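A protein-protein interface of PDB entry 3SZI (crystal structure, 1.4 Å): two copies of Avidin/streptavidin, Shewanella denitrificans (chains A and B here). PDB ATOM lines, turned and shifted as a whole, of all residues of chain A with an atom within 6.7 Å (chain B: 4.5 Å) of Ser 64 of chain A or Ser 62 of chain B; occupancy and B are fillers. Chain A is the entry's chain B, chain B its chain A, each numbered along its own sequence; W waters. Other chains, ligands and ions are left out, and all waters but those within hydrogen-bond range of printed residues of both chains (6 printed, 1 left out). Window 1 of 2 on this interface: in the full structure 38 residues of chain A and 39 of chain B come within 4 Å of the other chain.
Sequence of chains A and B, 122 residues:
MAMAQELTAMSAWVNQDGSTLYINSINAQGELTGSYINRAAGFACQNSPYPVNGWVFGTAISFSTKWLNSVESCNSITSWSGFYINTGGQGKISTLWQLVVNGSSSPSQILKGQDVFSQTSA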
ATOM      1  N   LEU A  32      23.819  23.870 -14.682  1.00  0.00           N
ATOM      2  CA  LEU A  32      23.883  22.612 -15.405  1.00  0.00           C
ATOM      3  C   LEU A  32      24.043  22.856 -16.886  1.00  0.00           C
ATOM      4  O   LEU A  32      23.467  23.796 -17.455  1.00  0.00           O
ATOM      5  CB  LEU A  32      22.604  21.795 -15.119  1.00  0.00           C
ATOM      6  CG  LEU A  32      22.258  20.526 -15.897  1.00  0.00           C
ATOM      7  CD1 LEU A  32      21.382  19.604 -15.066  1.00  0.00           C
ATOM      8  CD2 LEU A  32      21.595  20.813 -17.250  1.00  0.00           C
ATOM      9  N   TYR A  50      20.330  17.964 -28.652  1.00  0.00           N
ATOM     10  CA  TYR A  50      19.918  19.364 -28.437  1.00  0.00           C
ATOM     11  C   TYR A  50      20.562  19.840 -27.132  1.00  0.00           C
ATOM     12  O   TYR A  50      20.461  19.151 -26.116  1.00  0.00           O
ATOM     13  CB  TYR A  50      18.378  19.471 -28.374  1.00  0.00           C
ATOM     14  CG  TYR A  50      17.776  19.277 -29.752  1.00  0.00           C
ATOM     15  CD1 TYR A  50      17.464  18.006 -30.230  1.00  0.00           C
ATOM     16  CD2 TYR A  50      17.587  20.360 -30.606  1.00  0.00           C
ATOM     17  CE1 TYR A  50      16.971  17.811 -31.499  1.00  0.00           C
ATOM     18  CE2 TYR A  50      17.066  20.176 -31.882  1.00  0.00           C
ATOM     19  CZ  TYR A  50      16.770  18.895 -32.326  1.00  0.00           C
ATOM     20  OH  TYR A  50      16.286  18.639 -33.590  1.00  0.00           O
ATOM     21  N   PRO A  51      21.276  20.977 -27.144  1.00  0.00           N
ATOM     22  CA  PRO A  51      21.857  21.507 -25.909  1.00  0.00           C
ATOM     23  C   PRO A  51      20.849  21.818 -24.819  1.00  0.00           C
ATOM     24  O   PRO A  51      19.737  22.263 -25.095  1.00  0.00           O
ATOM     25  CB  PRO A  51      22.552  22.793 -26.372  1.00  0.00           C
ATOM     26  CG  PRO A  51      22.871  22.531 -27.781  1.00  0.00           C
ATOM     27  CD  PRO A  51      21.674  21.790 -28.303  1.00  0.00           C
ATOM     28  N   VAL A  52      21.291  21.598 -23.577  1.00  0.00           N
ATOM     29  CA  VAL A  52      20.477  21.793 -22.390  1.00  0.00           C
ATOM     30  C   VAL A  52      21.221  22.696 -21.417  1.00  0.00           C
ATOM     31  O   VAL A  52      22.437  22.569 -21.258  1.00  0.00           O
ATOM     32  CB  VAL A  52      20.225  20.429 -21.695  1.00  0.00           C
ATOM     33  CG1 VAL A  52      19.425  20.580 -20.414  1.00  0.00           C
ATOM     34  CG2 VAL A  52      19.541  19.463 -22.657  1.00  0.00           C
ATOM     35  N   ASN A  53      20.467  23.567 -20.752  1.00  0.00           N
ATOM     36  CA  ASN A  53      20.969  24.299 -19.605  1.00  0.00           C
ATOM     37  C   ASN A  53      19.969  24.162 -18.450  1.00  0.00           C
ATOM     38  O   ASN A  53      18.888  23.586 -18.614  1.00  0.00           O
ATOM     39  CB  ASN A  53      21.304  25.771 -19.946  1.00  0.00           C
ATOM     40  CG  ASN A  53      20.110  26.549 -20.445  1.00  0.00           C
ATOM     41  OD1 ASN A  53      18.948  26.214 -20.180  1.00  0.00           O
ATOM     42  ND2 ASN A  53      20.407  27.648 -21.141  1.00  0.00           N
ATOM     43  N   GLY A  54      20.342  24.625 -17.272  1.00  0.00           N
ATOM     44  CA  GLY A  54      19.440  24.475 -16.127  1.00  0.00           C
ATOM     45  C   GLY A  54      20.178  24.660 -14.821  1.00  0.00           C
ATOM     46  O   GLY A  54      21.254  25.274 -14.797  1.00  0.00           O
ATOM     47  N   SER A  62      16.037  21.868 -12.615  1.00  0.00           N
ATOM     48  CA  SER A  62      15.340  22.383 -13.797  1.00  0.00           C
ATOM     49  C   SER A  62      16.277  22.227 -14.970  1.00  0.00           C
ATOM     50  O   SER A  62      17.500  22.361 -14.843  1.00  0.00           O
ATOM     51  CB  SER A  62      14.957  23.842 -13.579  1.00  0.00           C
ATOM     52  OG  SER A  62      16.036  24.721 -13.847  1.00  0.00           O
ATOM     53  N   PHE A  63      15.718  21.885 -16.116  1.00  0.00           N
ATOM     54  CA  PHE A  63      16.522  21.912 -17.329  1.00  0.00           C
ATOM     55  C   PHE A  63      15.652  22.303 -18.491  1.00  0.00           C
ATOM     56  O   PHE A  63      14.447  22.087 -18.452  1.00  0.00           O
ATOM     57  CB  PHE A  63      17.330  20.607 -17.559  1.00  0.00           C
ATOM     58  CG  PHE A  63      16.499  19.350 -17.628  1.00  0.00           C
ATOM     59  CD1 PHE A  63      16.141  18.686 -16.473  1.00  0.00           C
ATOM     60  CD2 PHE A  63      16.104  18.821 -18.857  1.00  0.00           C
ATOM     61  CE1 PHE A  63      15.367  17.517 -16.515  1.00  0.00           C
ATOM     62  CE2 PHE A  63      15.331  17.631 -18.920  1.00  0.00           C
ATOM     63  CZ  PHE A  63      14.973  16.999 -17.736  1.00  0.00           C
ATOM     64  N   SER A  64      16.269  22.903 -19.499  1.00  0.00           N
ATOM     65  CA  SER A  64      15.528  23.420 -20.640  1.00  0.00           C
ATOM     66  C   SER A  64      16.310  23.234 -21.918  1.00  0.00           C
ATOM     67  O   SER A  64      17.551  23.314 -21.936  1.00  0.00           O
ATOM     68  CB  SER A  64      15.222  24.899 -20.463  1.00  0.00           C
ATOM     69  OG  SER A  64      14.372  25.108 -19.356  1.00  0.00           O
ATOM     70  N   THR A  65      15.576  22.978 -22.996  1.00  0.00           N
ATOM     71  CA  THR A  65      16.222  22.829 -24.293  1.00  0.00           C
ATOM     72  C   THR A  65      15.459  23.591 -25.351  1.00  0.00           C
ATOM     73  O   THR A  65      14.226  23.617 -25.329  1.00  0.00           O
ATOM     74  CB  THR A  65      16.396  21.345 -24.695  1.00  0.00           C
ATOM     75  OG1 THR A  65      17.328  21.232 -25.785  1.00  0.00           O
ATOM     76  CG2 THR A  65      15.082  20.748 -25.118  1.00  0.00           C
ATOM     77  N   LYS A  66      16.218  24.223 -26.232  1.00  0.00           N
ATOM     78  CA  LYS A  66      15.673  24.870 -27.432  1.00  0.00           C
ATOM     79  C   LYS A  66      15.722  23.864 -28.575  1.00  0.00           C
ATOM     80  O   LYS A  66      16.789  23.298 -28.845  1.00  0.00           O
ATOM     81  CB  LYS A  66      16.478  26.119 -27.762  1.00  0.00           C
ATOM     82  CG  LYS A  66      16.139  26.769 -29.096  1.00  0.00           C
ATOM     83  CD  LYS A  66      16.873  28.070 -29.273  1.00  0.00           C
ATOM     84  CE  LYS A  66      16.700  28.591 -30.691  1.00  0.00           C
ATOM     85  NZ  LYS A  66      17.243  29.983 -30.869  1.00  0.00           N
ATOM     86  N   ILE A  77      10.518  25.477 -27.356  1.00  0.00           N
ATOM     87  CA  ILE A  77      11.410  25.269 -26.208  1.00  0.00           C
ATOM     88  C   ILE A  77      10.678  24.457 -25.171  1.00  0.00           C
ATOM     89  O   ILE A  77       9.531  24.780 -24.868  1.00  0.00           O
ATOM     90  CB  ILE A  77      11.818  26.631 -25.559  1.00  0.00           C
ATOM     91  CG1 ILE A  77      12.502  27.543 -26.574  1.00  0.00           C
ATOM     92  CG2 ILE A  77      12.773  26.416 -24.402  1.00  0.00           C
ATOM     93  CD1 ILE A  77      12.567  29.018 -26.126  1.00  0.00           C
ATOM     94  N   THR A  78      11.347  23.436 -24.605  1.00  0.00           N
ATOM     95  CA  THR A  78      10.785  22.681 -23.503  1.00  0.00           C
ATOM     96  C   THR A  78      11.567  22.947 -22.228  1.00  0.00           C
ATOM     97  O   THR A  78      12.785  23.008 -22.266  1.00  0.00           O
ATOM     98  CB  THR A  78      10.748  21.151 -23.775  1.00  0.00           C
ATOM     99  OG1 THR A  78       9.935  20.926 -24.919  1.00  0.00           O
ATOM    100  CG2 THR A  78      10.151  20.377 -22.592  1.00  0.00           C
ATOM    101  N   SER A  79      10.838  23.103 -21.121  1.00  0.00           N
ATOM    102  CA  SER A  79      11.440  23.275 -19.812  1.00  0.00           C
ATOM    103  C   SER A  79      10.856  22.263 -18.865  1.00  0.00           C
ATOM    104  O   SER A  79       9.637  22.142 -18.743  1.00  0.00           O
ATOM    105  CB  SER A  79      11.123  24.669 -19.315  1.00  0.00           C
ATOM    106  OG  SER A  79      11.765  25.593 -20.138  1.00  0.00           O
ATOM    107  N   TRP A  80      11.748  21.564 -18.169  1.00  0.00           N
ATOM    108  CA  TRP A  80      11.372  20.592 -17.150  1.00  0.00           C
ATOM    109  C   TRP A  80      11.720  21.113 -15.761  1.00  0.00           C
ATOM    110  O   TRP A  80      12.778  21.739 -15.553  1.00  0.00           O
ATOM    111  CB  TRP A  80      12.170  19.318 -17.359  1.00  0.00           C
ATOM    112  CG  TRP A  80      11.868  18.488 -18.584  1.00  0.00           C
ATOM    113  CD1 TRP A  80      11.128  17.320 -18.626  1.00  0.00           C
ATOM    114  CD2 TRP A  80      12.402  18.668 -19.914  1.00  0.00           C
ATOM    115  NE1 TRP A  80      11.139  16.795 -19.894  1.00  0.00           N
ATOM    116  CE2 TRP A  80      11.915  17.590 -20.707  1.00  0.00           C
ATOM    117  CE3 TRP A  80      13.252  19.622 -20.512  1.00  0.00           C
ATOM    118  CZ2 TRP A  80      12.244  17.451 -22.065  1.00  0.00           C
ATOM    119  CZ3 TRP A  80      13.583  19.462 -21.864  1.00  0.00           C
ATOM    120  CH2 TRP A  80      13.080  18.394 -22.612  1.00  0.00           C
ATOM    121  N   GLN A  98       6.897  22.009 -19.569  1.00  0.00           N
ATOM    122  CA  GLN A  98       6.100  22.944 -20.351  1.00  0.00           C
ATOM    123  C   GLN A  98       6.809  23.163 -21.664  1.00  0.00           C
ATOM    124  O   GLN A  98       8.028  23.292 -21.706  1.00  0.00           O
ATOM    125  CB  GLN A  98       5.979  24.306 -19.651  1.00  0.00           C
ATOM    126  CG  GLN A  98       5.336  24.221 -18.278  1.00  0.00           C
ATOM    127  CD  GLN A  98       4.960  25.564 -17.724  1.00  0.00           C
ATOM    128  OE1 GLN A  98       5.812  26.423 -17.478  1.00  0.00           O
ATOM    129  NE2 GLN A  98       3.674  25.742 -17.492  1.00  0.00           N
ATOM    130  N   VAL A 100       6.738  25.654 -25.012  1.00  0.00           N
ATOM    131  CA  VAL A 100       6.220  26.874 -25.638  1.00  0.00           C
ATOM    132  C   VAL A 100       6.688  26.937 -27.068  1.00  0.00           C
ATOM    133  O   VAL A 100       7.868  26.732 -27.366  1.00  0.00           O
ATOM    134  CB  VAL A 100       6.607  28.148 -24.823  1.00  0.00           C
ATOM    135  CG1 VAL A 100       8.126  28.304 -24.666  1.00  0.00           C
ATOM    136  CG2 VAL A 100       5.961  29.401 -25.430  1.00  0.00           C
ATOM    137  N   ASN B  53      19.372  31.645 -16.446  1.00  0.00           N
ATOM    138  CA  ASN B  53      19.731  31.114 -17.759  1.00  0.00           C
ATOM    139  C   ASN B  53      18.444  30.741 -18.515  1.00  0.00           C
ATOM    140  O   ASN B  53      17.346  30.844 -17.965  1.00  0.00           O
ATOM    141  CB  ASN B  53      20.738  29.952 -17.669  1.00  0.00           C
ATOM    142  CG  ASN B  53      20.224  28.781 -16.850  1.00  0.00           C
ATOM    143  OD1 ASN B  53      19.023  28.580 -16.691  1.00  0.00           O
ATOM    144  ND2 ASN B  53      21.159  27.985 -16.329  1.00  0.00           N
ATOM    145  N   GLY B  54      18.565  30.395 -19.788  1.00  0.00           N
ATOM    146  CA  GLY B  54      17.391  30.015 -20.567  1.00  0.00           C
ATOM    147  C   GLY B  54      17.661  30.083 -22.044  1.00  0.00           C
ATOM    148  O   GLY B  54      18.810  30.001 -22.485  1.00  0.00           O
ATOM    149  N   TRP B  55      16.573  30.234 -22.791  1.00  0.00           N
ATOM    150  CA  TRP B  55      16.601  30.174 -24.253  1.00  0.00           C
ATOM    151  C   TRP B  55      15.583  31.114 -24.828  1.00  0.00           C
ATOM    152  O   TRP B  55      14.513  31.319 -24.229  1.00  0.00           O
ATOM    153  CB  TRP B  55      16.213  28.763 -24.737  1.00  0.00           C
ATOM    154  CG  TRP B  55      17.179  27.685 -24.321  1.00  0.00           C
ATOM    155  CD1 TRP B  55      17.001  26.765 -23.326  1.00  0.00           C
ATOM    156  CD2 TRP B  55      18.458  27.405 -24.917  1.00  0.00           C
ATOM    157  NE1 TRP B  55      18.114  25.959 -23.245  1.00  0.00           N
ATOM    158  CE2 TRP B  55      19.012  26.316 -24.224  1.00  0.00           C
ATOM    159  CE3 TRP B  55      19.174  27.967 -25.988  1.00  0.00           C
ATOM    160  CZ2 TRP B  55      20.277  25.778 -24.557  1.00  0.00           C
ATOM    161  CZ3 TRP B  55      20.429  27.437 -26.322  1.00  0.00           C
ATOM    162  CH2 TRP B  55      20.971  26.354 -25.591  1.00  0.00           C
ATOM    163  N   ILE B  61      10.253  32.050 -25.155  1.00  0.00           N
ATOM    164  CA  ILE B  61      11.341  32.228 -24.231  1.00  0.00           C
ATOM    165  C   ILE B  61      11.139  31.295 -23.042  1.00  0.00           C
ATOM    166  O   ILE B  61      10.003  31.089 -22.594  1.00  0.00           O
ATOM    167  CB  ILE B  61      11.461  33.710 -23.772  1.00  0.00           C
ATOM    168  CG1 ILE B  61      12.541  33.903 -22.709  1.00  0.00           C
ATOM    169  CG2 ILE B  61      10.117  34.239 -23.232  1.00  0.00           C
ATOM    170  CD1 ILE B  61      12.868  35.377 -22.399  1.00  0.00           C
ATOM    171  N   SER B  62      12.243  30.748 -22.549  1.00  0.00           N
ATOM    172  CA  SER B  62      12.236  30.126 -21.237  1.00  0.00           C
ATOM    173  C   SER B  62      13.359  30.723 -20.441  1.00  0.00           C
ATOM    174  O   SER B  62      14.418  31.057 -20.992  1.00  0.00           O
ATOM    175  CB  SER B  62      12.414  28.622 -21.334  1.00  0.00           C
ATOM    176  OG  SER B  62      12.408  28.053 -20.044  1.00  0.00           O
ATOM    177  N   PHE B  63      13.115  30.892 -19.147  1.00  0.00           N
ATOM    178  CA  PHE B  63      14.193  31.326 -18.280  1.00  0.00           C
ATOM    179  C   PHE B  63      13.998  30.702 -16.927  1.00  0.00           C
ATOM    180  O   PHE B  63      12.865  30.401 -16.541  1.00  0.00           O
ATOM    181  CB  PHE B  63      14.361  32.860 -18.228  1.00  0.00           C
ATOM    182  CG  PHE B  63      13.169  33.623 -17.759  1.00  0.00           C
ATOM    183  CD1 PHE B  63      12.187  34.015 -18.671  1.00  0.00           C
ATOM    184  CD2 PHE B  63      13.059  34.040 -16.435  1.00  0.00           C
ATOM    185  CE1 PHE B  63      11.082  34.765 -18.262  1.00  0.00           C
ATOM    186  CE2 PHE B  63      11.949  34.793 -16.035  1.00  0.00           C
ATOM    187  CZ  PHE B  63      10.970  35.155 -16.962  1.00  0.00           C
ATOM    188  N   SER B  64      15.113  30.444 -16.244  1.00  0.00           N
ATOM    189  CA  SER B  64      15.054  29.797 -14.943  1.00  0.00           C
ATOM    190  C   SER B  64      16.070  30.359 -13.994  1.00  0.00           C
ATOM    191  O   SER B  64      17.157  30.751 -14.406  1.00  0.00           O
ATOM    192  CB  SER B  64      15.302  28.296 -15.067  1.00  0.00           C
ATOM    193  OG  SER B  64      14.341  27.687 -15.898  1.00  0.00           O
ATOM    194  N   TRP B  80      10.287  29.696 -15.894  1.00  0.00           N
ATOM    195  CA  TRP B  80       9.206  30.365 -16.631  1.00  0.00           C
ATOM    196  C   TRP B  80       9.257  29.938 -18.079  1.00  0.00           C
ATOM    197  O   TRP B  80      10.345  29.841 -18.669  1.00  0.00           O
ATOM    198  CB  TRP B  80       9.413  31.873 -16.614  1.00  0.00           C
ATOM    199  CG  TRP B  80       9.236  32.608 -15.292  1.00  0.00           C
ATOM    200  CD1 TRP B  80       8.149  33.340 -14.913  1.00  0.00           C
ATOM    201  CD2 TRP B  80      10.215  32.773 -14.236  1.00  0.00           C
ATOM    202  NE1 TRP B  80       8.367  33.928 -13.677  1.00  0.00           N
ATOM    203  CE2 TRP B  80       9.620  33.575 -13.233  1.00  0.00           C
ATOM    204  CE3 TRP B  80      11.509  32.269 -14.022  1.00  0.00           C
ATOM    205  CZ2 TRP B  80      10.299  33.950 -12.066  1.00  0.00           C
ATOM    206  CZ3 TRP B  80      12.190  32.649 -12.856  1.00  0.00           C
ATOM    207  CH2 TRP B  80      11.572  33.470 -11.893  1.00  0.00           C
ATOM    208  N   SER B  81       8.075  29.681 -18.644  1.00  0.00           N
ATOM    209  CA  SER B  81       7.942  29.436 -20.076  1.00  0.00           C
ATOM    210  C   SER B  81       6.974  30.474 -20.602  1.00  0.00           C
ATOM    211  O   SER B  81       5.924  30.708 -19.999  1.00  0.00           O
ATOM    212  CB  SER B  81       7.364  28.036 -20.325  1.00  0.00           C
ATOM    213  OG  SER B  81       8.270  27.030 -19.905  1.00  0.00           O
HETATM  214  O   HOH W   1       8.658  26.409 -17.187  1.00  0.00           O
HETATM  215  O   HOH W   2      15.930  25.085 -16.700  1.00  0.00           O
HETATM  216  O   HOH W   3      17.319  27.063 -18.152  1.00  0.00           O
HETATM  217  O   HOH W   4      13.273  24.491 -16.638  1.00  0.00           O
HETATM  218  O   HOH W   5      14.801  28.132 -18.820  1.00  0.00           O
HETATM  219  O   HOH W   6       9.636  26.153 -22.006  1.00  0.00           O
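ND2 of Asn 53 of chain B sits at hydrogen-bond distance from O of Gly 54 of chain A. The backbone carbonyl oxygen of Gly 54 of chain B is in hydrogen-bond range of the side-chain amide nitrogen of Asn 53 of chain A (3.1 Å). The indole nitrogen (NE1) of Trp 55 of chain B lies within hydrogen-bond range of the side-chain amide oxygen (OD1) of Asn 53 of chain A (3.2 Å). NE1 of Trp 55 of chain B is in hydrogen-bond range of O of Ser 64 of chain A (3.0 Å). OG of Ser 79 of chain A is in hydrogen-bond range of OG of Ser 62 of chain B.
The side-chain hydroxyl (OG) of Ser 62 of chain B sits at hydrogen-bond distance from the backbone carbonyl oxygen (O) of Trp 80 of chain B (3.1 Å). The backbone carbonyl oxygen of Gly 54 of chain A is in hydrogen-bond range of the backbone NH of Leu 32 of chain A (2.9 Å). OG1 of Thr 65 of chain A is in hydrogen-bond range of O of Pro 51 of chain A (2.7 Å). OG of Ser 64 of chain A sits at hydrogen-bond distance from OG of Ser 79 of chain A. The backbone carbonyl oxygen of Thr 78 of chain A sits at hydrogen-bond distance from the backbone NH of Thr 65 of chain A (2.9 Å). The backbone NH (N) of Gln 98 of chain A is in hydrogen-bond range of the backbone carbonyl oxygen (O) of Ser 79 of chain A (2.9 Å).
Among the printed residues, merely in contact across the chains: Gln 98 of chain A with Ser 81 of chain B, Ile 77 of chain A with Trp 55 of chain B, Pro 51 of chain A with Trp 55 of chain B, Ser 64 of chain A with Ser 62 of chain B, Lys 66 of chain A with Trp 55 of chain B, Ser 79 of chain A with Ser 81 of chain B, Ile 77 of chain A with Ser 62 of chain B, Thr 65 of chain A with Trp 55 of chain B, Ser 62 of chain A with Ser 64 of chain B, Ile 77 of chain A with Ile 61 of chain B and Val 100 of chain A with Ile 61 of chain B.
Leu 32 of chain A touches none of the printed residues of chain B. Printed residues of chain B within 4 Å of Asn 53 of chain A: Gly 54 and Trp 55. Printed residues of chain B within 4 Å of Ser 64 of chain A: Trp 55 (3.0 Å) and Ser 62 (3.6 Å). Of the printed residues of chain B, Lys 66 of chain A touches Trp 55. Printed residues of chain B within 4 Å of Val 100 of chain A: Ile 61. Printed residues of chain A within 4 Å of Ile 61 of chain B: Ile 77 and Val 100. Printed residues of chain A within 4 Å of Ser 64 of chain B: Ser 62. The nearest printed residue of chain B that does not touch Thr 65 of chain A is Ser 62 of chain B (6.7 Å).
Of the 9 printed residues of chain B, 7 touch a printed residue of chain A. Hydrophobic or aromatic side chains of chain B within 4 Å of the printed part of chain A: Trp 55.
Asn 53 of chain A touches Gly 54 of chain B, and with the chains exchanged Gly 54 of chain A touches Asn 53 of chain B. Ser 62 of chain A touches Ser 64 of chain B, and with the chains exchanged Ser 64 of chain A touches Ser 62 of chain B. Positions printed for both chains: 53, 54, 62, 63, 64 and 80. Of the 16 pairs that touch across the chains among the printed residues, 4 have their exchanged pair printed and touching as well.
Water W6 lies within hydrogen-bond range of the side-chain hydroxyl (OG) of Ser 81 of chain B, the side-chain hydroxyl (OG) of Ser 79 of chain A, the backbone carbonyl oxygen (O) of Ile 77 of chain A and the backbone carbonyl oxygen (O) of Gln 98 of chain A. Water W5 lies within hydrogen-bond range of OG of Ser 62 of chain B (2.7 Å), OG of Ser 64 of chain B (3.0 Å), OG of Ser 64 of chain A (3.1 Å) and N of Phe 63 of chain B (3.3 Å). Water W3 bridges OD1 of Asn 53 of chain B (2.7 Å) and OD1 of Asn 53 of chain A (2.7 Å). Water W1 bridges the side-chain hydroxyl (OG) of Ser 81 of chain B (2.8 Å) and the side-chain amide oxygen (OE1) of Gln 98 of chain A (2.9 Å). Water W2 lies within hydrogen-bond range of OG of Ser 62 of chain A, OG of Ser 64 of chain A, OG of Ser 64 of chain B and N of Phe 63 of chain A. Water W4 lies within hydrogen-bond range of OG of Ser 64 of chain A (3.0 Å), O of Trp 80 of chain A (3.0 Å), O of Phe 63 of chain A (3.2 Å) and OG of Ser 64 of chain B (3.5 Å).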
